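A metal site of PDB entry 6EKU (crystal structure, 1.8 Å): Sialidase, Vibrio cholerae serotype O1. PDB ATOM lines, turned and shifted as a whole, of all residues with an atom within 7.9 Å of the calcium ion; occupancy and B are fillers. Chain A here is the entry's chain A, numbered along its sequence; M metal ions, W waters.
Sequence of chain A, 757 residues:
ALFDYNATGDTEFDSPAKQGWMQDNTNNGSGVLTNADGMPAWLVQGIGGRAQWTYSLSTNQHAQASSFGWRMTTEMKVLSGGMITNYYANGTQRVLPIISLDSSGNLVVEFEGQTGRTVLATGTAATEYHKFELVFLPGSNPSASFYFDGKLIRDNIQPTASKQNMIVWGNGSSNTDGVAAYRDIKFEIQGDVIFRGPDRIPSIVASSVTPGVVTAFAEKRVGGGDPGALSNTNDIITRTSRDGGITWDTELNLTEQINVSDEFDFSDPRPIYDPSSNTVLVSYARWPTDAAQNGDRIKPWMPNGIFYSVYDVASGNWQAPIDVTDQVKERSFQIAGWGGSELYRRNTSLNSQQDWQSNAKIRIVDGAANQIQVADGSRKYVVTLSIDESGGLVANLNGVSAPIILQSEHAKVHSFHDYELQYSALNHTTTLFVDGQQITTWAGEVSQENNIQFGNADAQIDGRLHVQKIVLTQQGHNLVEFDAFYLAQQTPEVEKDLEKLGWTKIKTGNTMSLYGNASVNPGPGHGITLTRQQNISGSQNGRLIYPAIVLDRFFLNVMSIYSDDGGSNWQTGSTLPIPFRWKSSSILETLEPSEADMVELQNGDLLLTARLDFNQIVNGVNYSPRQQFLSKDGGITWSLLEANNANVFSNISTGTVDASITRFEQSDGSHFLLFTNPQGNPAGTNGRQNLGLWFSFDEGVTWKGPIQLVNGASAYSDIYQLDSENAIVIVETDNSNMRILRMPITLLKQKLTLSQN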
ATOM      1  N   ILE A 201     -28.461  36.566 -15.178  1.00  0.00           N
ATOM      2  CA  ILE A 201     -28.400  35.089 -15.084  1.00  0.00           C
ATOM      3  C   ILE A 201     -29.791  34.436 -15.230  1.00  0.00           C
ATOM      4  O   ILE A 201     -30.337  33.870 -14.289  1.00  0.00           O
ATOM      5  CB  ILE A 201     -27.735  34.615 -13.757  1.00  0.00           C
ATOM      6  CG1 ILE A 201     -26.569  35.533 -13.363  1.00  0.00           C
ATOM      7  CG2 ILE A 201     -27.235  33.155 -13.904  1.00  0.00           C
ATOM      8  CD1 ILE A 201     -25.418  35.575 -14.330  1.00  0.00           C
ATOM      9  N   PRO A 202     -30.356  34.513 -16.447  1.00  0.00           N
ATOM     10  CA  PRO A 202     -31.738  34.073 -16.673  1.00  0.00           C
ATOM     11  C   PRO A 202     -31.924  32.592 -16.891  1.00  0.00           C
ATOM     12  O   PRO A 202     -31.047  31.904 -17.426  1.00  0.00           O
ATOM     13  CB  PRO A 202     -32.119  34.821 -17.960  1.00  0.00           C
ATOM     14  CG  PRO A 202     -30.841  34.895 -18.719  1.00  0.00           C
ATOM     15  CD  PRO A 202     -29.784  35.155 -17.632  1.00  0.00           C
ATOM     16  N   SER A 203     -33.103  32.110 -16.520  1.00  0.00           N
ATOM     17  CA  SER A 203     -33.489  30.731 -16.821  1.00  0.00           C
ATOM     18  C   SER A 203     -34.996  30.716 -17.013  1.00  0.00           C
ATOM     19  O   SER A 203     -35.687  31.643 -16.597  1.00  0.00           O
ATOM     20  CB  SER A 203     -33.053  29.783 -15.707  1.00  0.00           C
ATOM     21  OG  SER A 203     -33.600  30.164 -14.464  1.00  0.00           O
ATOM     22  N   ARG A 270     -31.986  27.528 -10.978  1.00  0.00           N
ATOM     23  CA  ARG A 270     -32.020  26.368 -11.863  1.00  0.00           C
ATOM     24  C   ARG A 270     -33.378  25.683 -11.744  1.00  0.00           C
ATOM     25  O   ARG A 270     -33.556  24.809 -10.889  1.00  0.00           O
ATOM     26  CB  ARG A 270     -30.876  25.409 -11.486  1.00  0.00           C
ATOM     27  CG  ARG A 270     -30.868  24.059 -12.216  1.00  0.00           C
ATOM     28  CD  ARG A 270     -30.276  24.174 -13.609  1.00  0.00           C
ATOM     29  NE  ARG A 270     -28.822  24.290 -13.581  1.00  0.00           N
ATOM     30  CZ  ARG A 270     -28.046  24.291 -14.656  1.00  0.00           C
ATOM     31  NH1 ARG A 270     -28.576  24.193 -15.889  1.00  0.00           N
ATOM     32  NH2 ARG A 270     -26.737  24.413 -14.503  1.00  0.00           N
ATOM     33  N   GLY A 523     -25.880  26.334 -10.809  1.00  0.00           N
ATOM     34  CA  GLY A 523     -25.455  26.829 -12.105  1.00  0.00           C
ATOM     35  C   GLY A 523     -26.642  27.336 -12.907  1.00  0.00           C
ATOM     36  O   GLY A 523     -27.794  27.047 -12.579  1.00  0.00           O
ATOM     37  N   PRO A 524     -26.361  28.071 -13.998  1.00  0.00           N
ATOM     38  CA  PRO A 524     -27.336  28.861 -14.769  1.00  0.00           C
ATOM     39  C   PRO A 524     -27.996  28.083 -15.909  1.00  0.00           C
ATOM     40  O   PRO A 524     -27.314  27.483 -16.716  1.00  0.00           O
ATOM     41  CB  PRO A 524     -26.477  29.991 -15.327  1.00  0.00           C
ATOM     42  CG  PRO A 524     -25.156  29.355 -15.573  1.00  0.00           C
ATOM     43  CD  PRO A 524     -24.979  28.302 -14.475  1.00  0.00           C
ATOM     44  N   GLY A 525     -29.323  28.117 -15.948  1.00  0.00           N
ATOM     45  CA  GLY A 525     -30.099  27.396 -16.927  1.00  0.00           C
ATOM     46  C   GLY A 525     -31.212  26.628 -16.250  1.00  0.00           C
ATOM     47  O   GLY A 525     -31.556  26.937 -15.118  1.00  0.00           O
ATOM     48  N   HIS A 526     -31.784  25.649 -16.949  1.00  0.00           N
ATOM     49  CA  HIS A 526     -32.809  24.805 -16.339  1.00  0.00           C
ATOM     50  C   HIS A 526     -32.274  23.387 -16.188  1.00  0.00           C
ATOM     51  O   HIS A 526     -31.231  23.050 -16.735  1.00  0.00           O
ATOM     52  CB  HIS A 526     -34.107  24.816 -17.156  1.00  0.00           C
ATOM     53  CG  HIS A 526     -33.941  24.421 -18.600  1.00  0.00           C
ATOM     54  ND1 HIS A 526     -33.813  25.344 -19.620  1.00  0.00           N
ATOM     55  CD2 HIS A 526     -33.908  23.203 -19.206  1.00  0.00           C
ATOM     56  CE1 HIS A 526     -33.687  24.717 -20.769  1.00  0.00           C
ATOM     57  NE2 HIS A 526     -33.745  23.415 -20.550  1.00  0.00           N
ATOM     58  N   PRO A 547     -27.104  19.778 -13.759  1.00  0.00           N
ATOM     59  CA  PRO A 547     -25.657  19.661 -13.663  1.00  0.00           C
ATOM     60  C   PRO A 547     -25.078  20.805 -12.836  1.00  0.00           C
ATOM     61  O   PRO A 547     -25.018  21.945 -13.286  1.00  0.00           O
ATOM     62  CB  PRO A 547     -25.206  19.720 -15.133  1.00  0.00           C
ATOM     63  CG  PRO A 547     -26.220  20.593 -15.785  1.00  0.00           C
ATOM     64  CD  PRO A 547     -27.509  20.486 -14.989  1.00  0.00           C
ATOM     65  N   GLU A 595     -20.355  26.220 -15.867  1.00  0.00           N
ATOM     66  CA  GLU A 595     -21.753  26.411 -16.207  1.00  0.00           C
ATOM     67  C   GLU A 595     -22.198  25.409 -17.263  1.00  0.00           C
ATOM     68  O   GLU A 595     -21.700  25.405 -18.386  1.00  0.00           O
ATOM     69  CB  GLU A 595     -21.975  27.839 -16.690  1.00  0.00           C
ATOM     70  CG  GLU A 595     -21.614  28.849 -15.616  1.00  0.00           C
ATOM     71  CD  GLU A 595     -21.750  30.269 -16.080  1.00  0.00           C
ATOM     72  OE1 GLU A 595     -21.675  30.495 -17.313  1.00  0.00           O
ATOM     73  OE2 GLU A 595     -21.939  31.162 -15.211  1.00  0.00           O
ATOM     74  N   ALA A 596     -23.147  24.554 -16.890  1.00  0.00           N
ATOM     75  CA  ALA A 596     -23.460  23.414 -17.742  1.00  0.00           C
ATOM     76  C   ALA A 596     -24.963  23.268 -17.939  1.00  0.00           C
ATOM     77  O   ALA A 596     -25.759  23.770 -17.133  1.00  0.00           O
ATOM     78  CB  ALA A 596     -22.844  22.119 -17.145  1.00  0.00           C
ATOM     79  N   ASP A 597     -25.344  22.587 -19.010  1.00  0.00           N
ATOM     80  CA  ASP A 597     -26.740  22.326 -19.349  1.00  0.00           C
ATOM     81  C   ASP A 597     -26.837  20.930 -19.947  1.00  0.00           C
ATOM     82  O   ASP A 597     -25.944  20.495 -20.665  1.00  0.00           O
ATOM     83  CB  ASP A 597     -27.265  23.395 -20.328  1.00  0.00           C
ATOM     84  CG  ASP A 597     -27.167  24.803 -19.751  1.00  0.00           C
ATOM     85  OD1 ASP A 597     -26.048  25.395 -19.785  1.00  0.00           O
ATOM     86  OD2 ASP A 597     -28.176  25.301 -19.224  1.00  0.00           O
ATOM     87  N   MET A 598     -27.915  20.223 -19.664  1.00  0.00           N
ATOM     88  CA  MET A 598     -28.039  18.868 -20.176  1.00  0.00           C
ATOM     89  C   MET A 598     -29.413  18.618 -20.797  1.00  0.00           C
ATOM     90  O   MET A 598     -30.401  19.293 -20.473  1.00  0.00           O
ATOM     91  CB  MET A 598     -27.788  17.830 -19.073  1.00  0.00           C
ATOM     92  CG  MET A 598     -28.940  17.670 -18.046  1.00  0.00           C
ATOM     93  SD  MET A 598     -28.662  16.275 -16.915  1.00  0.00           S
ATOM     94  CE  MET A 598     -27.160  16.829 -16.107  1.00  0.00           C
ATOM     95  N   THR A 609     -23.503  19.851 -22.012  1.00  0.00           N
ATOM     96  CA  THR A 609     -22.561  20.790 -22.591  1.00  0.00           C
ATOM     97  C   THR A 609     -22.102  21.731 -21.481  1.00  0.00           C
ATOM     98  O   THR A 609     -22.918  22.228 -20.707  1.00  0.00           O
ATOM     99  CB  THR A 609     -23.195  21.573 -23.785  1.00  0.00           C
ATOM    100  OG1 THR A 609     -22.227  22.458 -24.366  1.00  0.00           O
ATOM    101  CG2 THR A 609     -24.434  22.345 -23.374  1.00  0.00           C
ATOM    102  N   ARG A 626     -15.723  25.256 -24.537  1.00  0.00           N
ATOM    103  CA  ARG A 626     -16.916  24.451 -24.293  1.00  0.00           C
ATOM    104  C   ARG A 626     -16.641  22.992 -24.622  1.00  0.00           C
ATOM    105  O   ARG A 626     -15.921  22.699 -25.567  1.00  0.00           O
ATOM    106  CB  ARG A 626     -18.101  24.994 -25.121  1.00  0.00           C
ATOM    107  CG  ARG A 626     -19.406  24.203 -25.069  1.00  0.00           C
ATOM    108  CD  ARG A 626     -20.594  25.092 -25.539  1.00  0.00           C
ATOM    109  NE  ARG A 626     -20.740  26.223 -24.597  1.00  0.00           N
ATOM    110  CZ  ARG A 626     -21.352  26.152 -23.420  1.00  0.00           C
ATOM    111  NH1 ARG A 626     -21.911  25.006 -23.025  1.00  0.00           N
ATOM    112  NH2 ARG A 626     -21.401  27.215 -22.640  1.00  0.00           N
ATOM    113  N   VAL A 657     -18.898  31.695 -21.868  1.00  0.00           N
ATOM    114  CA  VAL A 657     -20.217  32.250 -21.589  1.00  0.00           C
ATOM    115  C   VAL A 657     -21.168  31.081 -21.338  1.00  0.00           C
ATOM    116  O   VAL A 657     -20.899  29.977 -21.795  1.00  0.00           O
ATOM    117  CB  VAL A 657     -20.719  33.119 -22.774  1.00  0.00           C
ATOM    118  CG1 VAL A 657     -21.037  32.235 -23.967  1.00  0.00           C
ATOM    119  CG2 VAL A 657     -21.934  33.950 -22.371  1.00  0.00           C
ATOM    120  N   ASP A 658     -22.236  31.298 -20.578  1.00  0.00           N
ATOM    121  CA  ASP A 658     -23.249  30.264 -20.391  1.00  0.00           C
ATOM    122  C   ASP A 658     -24.031  30.066 -21.680  1.00  0.00           C
ATOM    123  O   ASP A 658     -24.336  31.031 -22.391  1.00  0.00           O
ATOM    124  CB  ASP A 658     -24.231  30.639 -19.273  1.00  0.00           C
ATOM    125  CG  ASP A 658     -25.291  29.574 -19.057  1.00  0.00           C
ATOM    126  OD1 ASP A 658     -24.930  28.378 -18.967  1.00  0.00           O
ATOM    127  OD2 ASP A 658     -26.496  29.919 -18.951  1.00  0.00           O
ATOM    128  N   ALA A 659     -24.363  28.802 -21.947  1.00  0.00           N
ATOM    129  CA  ALA A 659     -25.188  28.428 -23.094  1.00  0.00           C
ATOM    130  C   ALA A 659     -26.487  27.776 -22.611  1.00  0.00           C
ATOM    131  O   ALA A 659     -26.755  27.715 -21.410  1.00  0.00           O
ATOM    132  CB  ALA A 659     -24.432  27.478 -24.020  1.00  0.00           C
ATOM    133  N   SER A 660     -27.285  27.298 -23.539  1.00  0.00           N
ATOM    134  CA  SER A 660     -28.497  26.563 -23.193  1.00  0.00           C
ATOM    135  C   SER A 660     -28.677  25.447 -24.214  1.00  0.00           C
ATOM    136  O   SER A 660     -28.344  25.611 -25.387  1.00  0.00           O
ATOM    137  CB  SER A 660     -29.724  27.473 -23.179  1.00  0.00           C
ATOM    138  OG  SER A 660     -30.914  26.773 -22.836  1.00  0.00           O
ATOM    139  N   ILE A 661     -29.200  24.317 -23.762  1.00  0.00           N
ATOM    140  CA  ILE A 661     -29.530  23.227 -24.684  1.00  0.00           C
ATOM    141  C   ILE A 661     -30.871  22.671 -24.240  1.00  0.00           C
ATOM    142  O   ILE A 661     -31.185  22.684 -23.048  1.00  0.00           O
ATOM    143  CB  ILE A 661     -28.428  22.155 -24.690  1.00  0.00           C
ATOM    144  CG1 ILE A 661     -28.657  21.144 -25.830  1.00  0.00           C
ATOM    145  CG2 ILE A 661     -28.344  21.440 -23.315  1.00  0.00           C
ATOM    146  CD1 ILE A 661     -27.446  20.203 -26.080  1.00  0.00           C
ATOM    147  N   THR A 676     -28.474  27.484 -27.741  1.00  0.00           N
ATOM    148  CA  THR A 676     -28.279  28.943 -27.905  1.00  0.00           C
ATOM    149  C   THR A 676     -27.006  29.436 -27.209  1.00  0.00           C
ATOM    150  O   THR A 676     -26.620  28.934 -26.148  1.00  0.00           O
ATOM    151  CB  THR A 676     -29.501  29.770 -27.362  1.00  0.00           C
ATOM    152  OG1 THR A 676     -29.774  29.439 -25.993  1.00  0.00           O
ATOM    153  CG2 THR A 676     -30.750  29.527 -28.190  1.00  0.00           C
ATOM    154  N   TYR A 716     -25.740  35.601 -21.492  1.00  0.00           N
ATOM    155  CA  TYR A 716     -26.389  34.371 -21.014  1.00  0.00           C
ATOM    156  C   TYR A 716     -27.786  34.240 -21.632  1.00  0.00           C
ATOM    157  O   TYR A 716     -28.476  35.235 -21.832  1.00  0.00           O
ATOM    158  CB  TYR A 716     -26.510  34.334 -19.491  1.00  0.00           C
ATOM    159  CG  TYR A 716     -25.227  34.082 -18.735  1.00  0.00           C
ATOM    160  CD1 TYR A 716     -23.989  34.461 -19.250  1.00  0.00           C
ATOM    161  CD2 TYR A 716     -25.255  33.447 -17.489  1.00  0.00           C
ATOM    162  CE1 TYR A 716     -22.819  34.233 -18.546  1.00  0.00           C
ATOM    163  CE2 TYR A 716     -24.075  33.209 -16.767  1.00  0.00           C
ATOM    164  CZ  TYR A 716     -22.871  33.589 -17.315  1.00  0.00           C
ATOM    165  OH  TYR A 716     -21.709  33.346 -16.648  1.00  0.00           O
ATOM    166  N   SER A 717     -28.183  33.002 -21.908  1.00  0.00           N
ATOM    167  CA  SER A 717     -29.498  32.741 -22.492  1.00  0.00           C
ATOM    168  C   SER A 717     -30.032  31.411 -22.019  1.00  0.00           C
ATOM    169  O   SER A 717     -29.268  30.554 -21.544  1.00  0.00           O
ATOM    170  CB  SER A 717     -29.416  32.749 -24.027  1.00  0.00           C
ATOM    171  OG  SER A 717     -28.681  31.614 -24.461  1.00  0.00           O
ATOM    172  N   ASP A 718     -31.334  31.212 -22.156  1.00  0.00           N
ATOM    173  CA  ASP A 718     -31.951  29.915 -21.868  1.00  0.00           C
ATOM    174  C   ASP A 718     -33.129  29.688 -22.828  1.00  0.00           C
ATOM    175  O   ASP A 718     -33.932  30.597 -23.052  1.00  0.00           O
ATOM    176  CB  ASP A 718     -32.408  29.840 -20.399  1.00  0.00           C
ATOM    177  CG  ASP A 718     -32.538  28.399 -19.898  1.00  0.00           C
ATOM    178  OD1 ASP A 718     -31.691  27.568 -20.291  1.00  0.00           O
ATOM    179  OD2 ASP A 718     -33.474  28.101 -19.134  1.00  0.00           O
ATOM    180  N   ILE A 719     -33.213  28.491 -23.408  1.00  0.00           N
ATOM    181  CA  ILE A 719     -34.271  28.175 -24.381  1.00  0.00           C
ATOM    182  C   ILE A 719     -35.074  26.968 -23.887  1.00  0.00           C
ATOM    183  O   ILE A 719     -34.515  26.041 -23.298  1.00  0.00           O
ATOM    184  CB  ILE A 719     -33.688  27.923 -25.795  1.00  0.00           C
ATOM    185  CG1 ILE A 719     -34.803  27.729 -26.834  1.00  0.00           C
ATOM    186  CG2 ILE A 719     -32.724  26.718 -25.775  1.00  0.00           C
ATOM    187  CD1 ILE A 719     -34.335  27.817 -28.291  1.00  0.00           C
HETATM  188 CA    CA M   1     -26.970  27.448 -19.068  1.00  0.00          CA
HETATM  189  O   HOH W   1     -29.101  28.495 -19.728  1.00  0.00           O
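The side-chain carboxylate (OE1) of Glu 595 lies close to the backbone NH (N) of Asp 658 (3.4 Å).
The side-chain carboxylate of Asp 597 lies close to the guanidinium group of Arg 270, at 3.5 Å.
The backbone NH (N) of Thr 609 lies within hydrogen-bond range of the backbone carbonyl oxygen (O) of Asp 597 (2.9 Å).
Gly 525 touches the calcium ion (CA to CA, 3.8 Å).
Five residues have an atom within 4 Å of the calcium ion: Pro 524, Gly 525, Asp 597, Asp 658 and Ala 659.
Along chain A the residues within 4 Å of the calcium ion span positions 524 to 659.
The nearest printed residue that does not touch the calcium ion is Ala 596 (4.3 Å).
OD1 of Asp 658 is bound to the calcium ion (2.2 Å).
The calcium ion is bound by OD1 of Asp 597.
The calcium ion is bound by O of Ala 659 (2.4 Å).
O of Pro 524 is bound to the calcium ion (2.4 Å).
The calcium ion is bound by water W1 (2.5 Å).
The calcium ion is bound by OD2 of Asp 597 (2.5 Å).
The side-chain carboxylate (OD2) of Asp 658 binds the calcium ion.
Water W1 bridges O of Ser 717 (2.8 Å) and OD1 of Asp 718 (2.8 Å).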
